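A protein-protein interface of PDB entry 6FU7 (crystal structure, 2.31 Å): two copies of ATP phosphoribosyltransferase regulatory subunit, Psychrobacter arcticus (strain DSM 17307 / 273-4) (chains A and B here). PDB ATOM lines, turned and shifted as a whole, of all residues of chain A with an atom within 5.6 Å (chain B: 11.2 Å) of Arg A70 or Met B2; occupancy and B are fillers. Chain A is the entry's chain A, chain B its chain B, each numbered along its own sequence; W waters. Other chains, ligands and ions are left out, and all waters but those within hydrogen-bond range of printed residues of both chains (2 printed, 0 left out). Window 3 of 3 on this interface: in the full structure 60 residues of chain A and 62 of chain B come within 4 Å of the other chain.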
ATOM      1  N   PHE A  44      16.198  -4.855   6.804  1.00  0.00           N
ATOM      2  CA  PHE A  44      14.838  -5.339   7.012  1.00  0.00           C
ATOM      3  C   PHE A  44      14.741  -6.720   6.366  1.00  0.00           C
ATOM      4  O   PHE A  44      15.390  -6.982   5.340  1.00  0.00           O
ATOM      5  CB  PHE A  44      13.820  -4.378   6.420  1.00  0.00           C
ATOM      6  CG  PHE A  44      13.753  -3.055   7.129  1.00  0.00           C
ATOM      7  CD1 PHE A  44      13.456  -2.994   8.479  1.00  0.00           C
ATOM      8  CD2 PHE A  44      13.968  -1.864   6.446  1.00  0.00           C
ATOM      9  CE1 PHE A  44      13.378  -1.775   9.145  1.00  0.00           C
ATOM     10  CE2 PHE A  44      13.888  -0.642   7.101  1.00  0.00           C
ATOM     11  CZ  PHE A  44      13.594  -0.597   8.459  1.00  0.00           C
ATOM     12  N   GLU A  46      12.258  -7.989   4.815  1.00  0.00           N
ATOM     13  CA  GLU A  46      11.615  -7.818   3.506  1.00  0.00           C
ATOM     14  C   GLU A  46      12.616  -7.868   2.349  1.00  0.00           C
ATOM     15  O   GLU A  46      12.319  -8.465   1.316  1.00  0.00           O
ATOM     16  CB  GLU A  46      10.820  -6.500   3.436  1.00  0.00           C
ATOM     17  CG  GLU A  46       9.430  -6.539   4.070  1.00  0.00           C
ATOM     18  CD  GLU A  46       9.422  -6.583   5.597  1.00  0.00           C
ATOM     19  OE1 GLU A  46      10.428  -6.193   6.230  1.00  0.00           O
ATOM     20  OE2 GLU A  46       8.401  -7.015   6.178  1.00  0.00           O
ATOM     21  N   SER A  47      13.792  -7.251   2.516  1.00  0.00           N
ATOM     22  CA  SER A  47      14.830  -7.294   1.476  1.00  0.00           C
ATOM     23  C   SER A  47      15.792  -8.467   1.666  1.00  0.00           C
ATOM     24  O   SER A  47      16.128  -9.153   0.700  1.00  0.00           O
ATOM     25  CB  SER A  47      15.588  -5.960   1.379  1.00  0.00           C
ATOM     26  OG  SER A  47      16.468  -5.755   2.467  1.00  0.00           O
ATOM     27  N   ILE A  63      15.958  -9.578  14.776  1.00  0.00           N
ATOM     28  CA  ILE A  63      16.050  -8.513  15.762  1.00  0.00           C
ATOM     29  C   ILE A  63      15.024  -7.454  15.368  1.00  0.00           C
ATOM     30  O   ILE A  63      14.634  -7.379  14.204  1.00  0.00           O
ATOM     31  CB  ILE A  63      17.470  -7.903  15.816  1.00  0.00           C
ATOM     32  CG1 ILE A  63      17.955  -7.492  14.421  1.00  0.00           C
ATOM     33  CG2 ILE A  63      18.469  -8.888  16.434  1.00  0.00           C
ATOM     34  CD1 ILE A  63      19.238  -6.683  14.413  1.00  0.00           C
ATOM     35  N   ILE A  64      14.593  -6.648  16.329  1.00  0.00           N
ATOM     36  CA  ILE A  64      13.545  -5.652  16.092  1.00  0.00           C
ATOM     37  C   ILE A  64      14.134  -4.244  15.959  1.00  0.00           C
ATOM     38  O   ILE A  64      14.960  -3.843  16.770  1.00  0.00           O
ATOM     39  CB  ILE A  64      12.462  -5.705  17.203  1.00  0.00           C
ATOM     40  CG1 ILE A  64      11.169  -5.068  16.693  1.00  0.00           C
ATOM     41  CG2 ILE A  64      12.911  -5.091  18.533  1.00  0.00           C
ATOM     42  CD1 ILE A  64      10.340  -6.024  15.863  1.00  0.00           C
ATOM     43  N   ASP A  65      13.715  -3.501  14.937  1.00  0.00           N
ATOM     44  CA  ASP A  65      14.129  -2.106  14.777  1.00  0.00           C
ATOM     45  C   ASP A  65      13.278  -1.246  15.707  1.00  0.00           C
ATOM     46  O   ASP A  65      12.088  -1.135  15.503  1.00  0.00           O
ATOM     47  CB  ASP A  65      13.950  -1.657  13.325  1.00  0.00           C
ATOM     48  CG  ASP A  65      14.354  -0.195  13.089  1.00  0.00           C
ATOM     49  OD1 ASP A  65      15.171   0.361  13.857  1.00  0.00           O
ATOM     50  OD2 ASP A  65      13.859   0.389  12.099  1.00  0.00           O
ATOM     51  N   THR A  68      11.215   1.824  13.997  1.00  0.00           N
ATOM     52  CA  THR A  68      10.000   1.533  13.206  1.00  0.00           C
ATOM     53  C   THR A  68       9.115   0.393  13.732  1.00  0.00           C
ATOM     54  O   THR A  68       7.972   0.252  13.287  1.00  0.00           O
ATOM     55  CB  THR A  68      10.358   1.186  11.744  1.00  0.00           C
ATOM     56  OG1 THR A  68      11.063  -0.066  11.691  1.00  0.00           O
ATOM     57  CG2 THR A  68      11.211   2.285  11.113  1.00  0.00           C
ATOM     58  N   GLY A  69       9.630  -0.412  14.658  1.00  0.00           N
ATOM     59  CA  GLY A  69       8.946  -1.616  15.108  1.00  0.00           C
ATOM     60  C   GLY A  69       8.966  -2.775  14.119  1.00  0.00           C
ATOM     61  O   GLY A  69       8.275  -3.768  14.339  1.00  0.00           O
ATOM     62  N   ARG A  70       9.765  -2.678  13.051  1.00  0.00           N
ATOM     63  CA  ARG A  70       9.825  -3.722  12.024  1.00  0.00           C
ATOM     64  C   ARG A  70      10.917  -4.742  12.323  1.00  0.00           C
ATOM     65  O   ARG A  70      11.859  -4.474  13.078  1.00  0.00           O
ATOM     66  CB  ARG A  70      10.069  -3.114  10.643  1.00  0.00           C
ATOM     67  CG  ARG A  70       8.951  -2.196  10.164  1.00  0.00           C
ATOM     68  CD  ARG A  70       9.308  -1.489   8.869  1.00  0.00           C
ATOM     69  NE  ARG A  70       9.674  -2.441   7.831  1.00  0.00           N
ATOM     70  CZ  ARG A  70      10.235  -2.136   6.661  1.00  0.00           C
ATOM     71  NH1 ARG A  70      10.502  -0.874   6.332  1.00  0.00           N
ATOM     72  NH2 ARG A  70      10.528  -3.121   5.806  1.00  0.00           N
ATOM     73  N   LEU A  71      10.785  -5.906  11.698  1.00  0.00           N
ATOM     74  CA  LEU A  71      11.753  -6.980  11.852  1.00  0.00           C
ATOM     75  C   LEU A  71      12.977  -6.736  10.984  1.00  0.00           C
ATOM     76  O   LEU A  71      12.854  -6.360   9.828  1.00  0.00           O
ATOM     77  CB  LEU A  71      11.151  -8.331  11.467  1.00  0.00           C
ATOM     78  CG  LEU A  71      10.110  -8.994  12.373  1.00  0.00           C
ATOM     79  CD1 LEU A  71       9.678 -10.316  11.745  1.00  0.00           C
ATOM     80  CD2 LEU A  71      10.627  -9.211  13.792  1.00  0.00           C
ATOM     81  N   MET A  72      14.158  -6.968  11.552  1.00  0.00           N
ATOM     82  CA  MET A  72      15.390  -7.017  10.782  1.00  0.00           C
ATOM     83  C   MET A  72      16.015  -8.384  10.951  1.00  0.00           C
ATOM     84  O   MET A  72      15.547  -9.181  11.740  1.00  0.00           O
ATOM     85  CB  MET A  72      16.350  -5.923  11.232  1.00  0.00           C
ATOM     86  CG  MET A  72      15.817  -4.505  11.092  1.00  0.00           C
ATOM     87  SD  MET A  72      17.016  -3.227  11.523  1.00  0.00           S
ATOM     88  CE  MET A  72      17.208  -3.453  13.294  1.00  0.00           C
ATOM     89  N   MET B   2      14.740  -0.184   0.529  1.00  0.00           N
ATOM     90  CA  MET B   2      14.956   0.757   1.672  1.00  0.00           C
ATOM     91  C   MET B   2      15.658   0.051   2.847  1.00  0.00           C
ATOM     92  O   MET B   2      15.139  -0.914   3.402  1.00  0.00           O
ATOM     93  CB  MET B   2      13.623   1.342   2.130  1.00  0.00           C
ATOM     94  CG  MET B   2      13.691   2.388   3.250  1.00  0.00           C
ATOM     95  SD  MET B   2      12.116   3.190   3.705  1.00  0.00           S
ATOM     96  CE  MET B   2      10.936   1.838   3.775  1.00  0.00           C
ATOM     97  N   LEU B   3      16.837   0.533   3.209  1.00  0.00           N
ATOM     98  CA  LEU B   3      17.555   0.038   4.387  1.00  0.00           C
ATOM     99  C   LEU B   3      17.039   0.741   5.643  1.00  0.00           C
ATOM    100  O   LEU B   3      16.435   1.797   5.531  1.00  0.00           O
ATOM    101  CB  LEU B   3      19.061   0.258   4.228  1.00  0.00           C
ATOM    102  CG  LEU B   3      19.689  -0.399   3.001  1.00  0.00           C
ATOM    103  CD1 LEU B   3      21.164  -0.028   2.897  1.00  0.00           C
ATOM    104  CD2 LEU B   3      19.527  -1.912   3.054  1.00  0.00           C
ATOM    105  N   PRO B   4      17.257   0.156   6.832  1.00  0.00           N
ATOM    106  CA  PRO B   4      16.927   0.850   8.083  1.00  0.00           C
ATOM    107  C   PRO B   4      17.753   2.120   8.294  1.00  0.00           C
ATOM    108  O   PRO B   4      18.864   2.229   7.773  1.00  0.00           O
ATOM    109  CB  PRO B   4      17.287  -0.179   9.173  1.00  0.00           C
ATOM    110  CG  PRO B   4      17.356  -1.498   8.482  1.00  0.00           C
ATOM    111  CD  PRO B   4      17.785  -1.201   7.081  1.00  0.00           C
ATOM    112  N   ASP B   5      17.224   3.060   9.073  1.00  0.00           N
ATOM    113  CA  ASP B   5      17.944   4.292   9.375  1.00  0.00           C
ATOM    114  C   ASP B   5      19.292   3.961  10.003  1.00  0.00           C
ATOM    115  O   ASP B   5      19.401   3.021  10.795  1.00  0.00           O
ATOM    116  CB  ASP B   5      17.143   5.204  10.312  1.00  0.00           C
ATOM    117  CG  ASP B   5      15.898   5.792   9.653  1.00  0.00           C
ATOM    118  OD1 ASP B   5      15.736   5.657   8.414  1.00  0.00           O
ATOM    119  OD2 ASP B   5      15.067   6.375  10.387  1.00  0.00           O
ATOM    120  N   GLY B   6      20.317   4.716   9.616  1.00  0.00           N
ATOM    121  CA  GLY B   6      21.674   4.446  10.040  1.00  0.00           C
ATOM    122  C   GLY B   6      22.323   3.190   9.481  1.00  0.00           C
ATOM    123  O   GLY B   6      23.264   2.672  10.073  1.00  0.00           O
ATOM    124  N   VAL B   7      21.820   2.707   8.348  1.00  0.00           N
ATOM    125  CA  VAL B   7      22.344   1.518   7.711  1.00  0.00           C
ATOM    126  C   VAL B   7      22.446   1.829   6.213  1.00  0.00           C
ATOM    127  O   VAL B   7      21.447   2.173   5.566  1.00  0.00           O
ATOM    128  CB  VAL B   7      21.441   0.290   7.938  1.00  0.00           C
ATOM    129  CG1 VAL B   7      22.065  -0.949   7.308  1.00  0.00           C
ATOM    130  CG2 VAL B   7      21.179   0.058   9.424  1.00  0.00           C
ATOM    131  N   ALA B   8      23.650   1.697   5.667  1.00  0.00           N
ATOM    132  CA  ALA B   8      23.926   2.061   4.285  1.00  0.00           C
ATOM    133  C   ALA B   8      24.852   1.035   3.667  1.00  0.00           C
ATOM    134  O   ALA B   8      25.755   0.548   4.339  1.00  0.00           O
ATOM    135  CB  ALA B   8      24.570   3.438   4.228  1.00  0.00           C
ATOM    136  N   ASP B   9      24.626   0.722   2.394  1.00  0.00           N
ATOM    137  CA  ASP B   9      25.628   0.026   1.580  1.00  0.00           C
ATOM    138  C   ASP B   9      26.875   0.899   1.451  1.00  0.00           C
ATOM    139  O   ASP B   9      26.778   2.130   1.438  1.00  0.00           O
ATOM    140  CB  ASP B   9      25.099  -0.208   0.153  1.00  0.00           C
ATOM    141  CG  ASP B   9      23.966  -1.207   0.095  1.00  0.00           C
ATOM    142  OD1 ASP B   9      24.058  -2.252   0.768  1.00  0.00           O
ATOM    143  OD2 ASP B   9      22.982  -0.956  -0.645  1.00  0.00           O
ATOM    144  N   PHE B  61      21.888  -5.456  20.719  1.00  0.00           N
ATOM    145  CA  PHE B  61      20.826  -6.367  20.268  1.00  0.00           C
ATOM    146  C   PHE B  61      20.952  -7.714  20.964  1.00  0.00           C
ATOM    147  O   PHE B  61      22.064  -8.237  21.087  1.00  0.00           O
ATOM    148  CB  PHE B  61      20.894  -6.606  18.742  1.00  0.00           C
ATOM    149  CG  PHE B  61      20.307  -5.488  17.923  1.00  0.00           C
ATOM    150  CD1 PHE B  61      18.939  -5.336  17.842  1.00  0.00           C
ATOM    151  CD2 PHE B  61      21.121  -4.591  17.235  1.00  0.00           C
ATOM    152  CE1 PHE B  61      18.385  -4.308  17.102  1.00  0.00           C
ATOM    153  CE2 PHE B  61      20.563  -3.552  16.497  1.00  0.00           C
ATOM    154  CZ  PHE B  61      19.199  -3.414  16.426  1.00  0.00           C
ATOM    155  N   THR B 106      21.703  -0.592  18.477  1.00  0.00           N
ATOM    156  CA  THR B 106      20.231  -0.543  18.398  1.00  0.00           C
ATOM    157  C   THR B 106      19.710   0.854  18.015  1.00  0.00           C
ATOM    158  O   THR B 106      18.725   0.959  17.284  1.00  0.00           O
ATOM    159  CB  THR B 106      19.571  -1.000  19.720  1.00  0.00           C
ATOM    160  OG1 THR B 106      20.001  -0.166  20.783  1.00  0.00           O
ATOM    161  CG2 THR B 106      19.925  -2.461  20.064  1.00  0.00           C
ATOM    162  N   ARG B 115      24.452   3.060  12.573  1.00  0.00           N
ATOM    163  CA  ARG B 115      24.192   1.976  13.507  1.00  0.00           C
ATOM    164  C   ARG B 115      25.074   0.754  13.232  1.00  0.00           C
ATOM    165  O   ARG B 115      24.954  -0.250  13.923  1.00  0.00           O
ATOM    166  CB  ARG B 115      22.715   1.568  13.439  1.00  0.00           C
ATOM    167  CG  ARG B 115      21.800   2.515  14.216  1.00  0.00           C
ATOM    168  CD  ARG B 115      20.443   1.894  14.512  1.00  0.00           C
ATOM    169  NE  ARG B 115      19.559   1.835  13.345  1.00  0.00           N
ATOM    170  CZ  ARG B 115      18.354   1.275  13.340  1.00  0.00           C
ATOM    171  NH1 ARG B 115      17.857   0.708  14.440  1.00  0.00           N
ATOM    172  NH2 ARG B 115      17.628   1.288  12.226  1.00  0.00           N
HETATM  173  O   HOH W   1      16.357  -3.424   4.340  1.00  0.00           O
HETATM  174  O   HOH W   2      12.699  -3.142   3.214  1.00  0.00           O
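The guanidinium group (NH1) of Arg B115 lies within salt-bridge range of the side-chain carboxylate (OD1) of Asp A65, at 2.8 Å.
The backbone carbonyl oxygen (O) of Thr B106 is in hydrogen-bond range of the guanidinium group (NH1) of Arg B115 (3.0 Å). The backbone carbonyl oxygen (O) of Phe A44 lies within hydrogen-bond range of the side-chain hydroxyl (OG) of Ser A47 (3.3 Å). The backbone carbonyl oxygen of Asp B5 is in hydrogen-bond range of the guanidinium group of Arg B115 (2.8 Å). OG1 of Thr A68 is in hydrogen-bond range of OD2 of Asp A65 (2.9 Å). The backbone NH (N) of Asp A65 lies within hydrogen-bond range of the backbone carbonyl oxygen (O) of Arg A70 (2.8 Å). The side-chain carboxylate (OE1) of Glu A46 lies within salt-bridge range of the guanidinium group (NH2) of Arg A70 (3.1 Å).
Met B2 touches Phe A44. Leu B3 touches Phe A44. Phe A44 touches Pro B4. Phe B61 touches Ile A63. O of Ile A64 touches CE1 of Phe B61, at 3.5 Å. Arg A70 touches Met B2 (NH1 to CE, 3.8 Å). Met A72 touches Pro B4 (SD to CG, 3.5 Å). CE of Met A72 touches CZ of Phe B61, 3.7 Å away.
Phe A44 touches three residues of chain B. Printed residues of chain B within 4 Å of Ile A64: Phe B61. Asp A65 touches just one residue of chain B: Arg B115 (2.8 Å). No residue of chain B comes within 4 Å of Thr A68. No residue of chain B comes within 4 Å of Gly A69. Of the printed residues of chain B, Arg A70 touches Met B2. Of chain B, only Pro B4 (3.5 Å) and Phe B61 (3.7 Å) come within 4 Å of Met A72. Met B2 touches two residues of chain A. Of the printed residues of chain A, Pro B4 touches Phe A44 (3.5 Å) and Met A72 (3.5 Å). Of the printed residues of chain A, Phe B61 touches Ile A63, Ile A64 and Met A72. Thr B106 touches none of the printed residues of chain A. The nearest residue of chain B that does not touch Arg A70 is Leu B3 (6.6 Å). The nearest residue of chain A that does not touch Met B2 is Ser A47 (5.1 Å).
Of the 11 printed residues of chain B, 5 touch a printed residue of chain A. Along chain B the printed residues that touch a printed residue of chain A span positions 2 to 115. Of the 11 printed residues of chain A, 6 touch a printed residue of chain B. Printed residues of chain A that touch a printed residue of chain B: Phe A44, Ile A63, Ile A64, Asp A65, Arg A70 and Met A72. Hydrophobic or aromatic side chains of chain A that line the printed part of chain B: Phe A44, Ile A63 and Met A72. Among the printed residues, Asp or Glu carboxylates within 4 Å of a Lys or Arg side-chain nitrogen of the other chain: Asp A65 with Arg B115 (2.8 Å).
No position is printed for both chains. Of the 9 pairs that touch across the chains among the printed residues, none has its exchanged pair printed and touching as well.
Water W1 lies within hydrogen-bond range of N of Phe A44, O of Met B2 and OG of Ser A47. Water W2 lies within hydrogen-bond range of O of Met B2 (3.3 Å) and NH2 of Arg A70 (3.4 Å).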
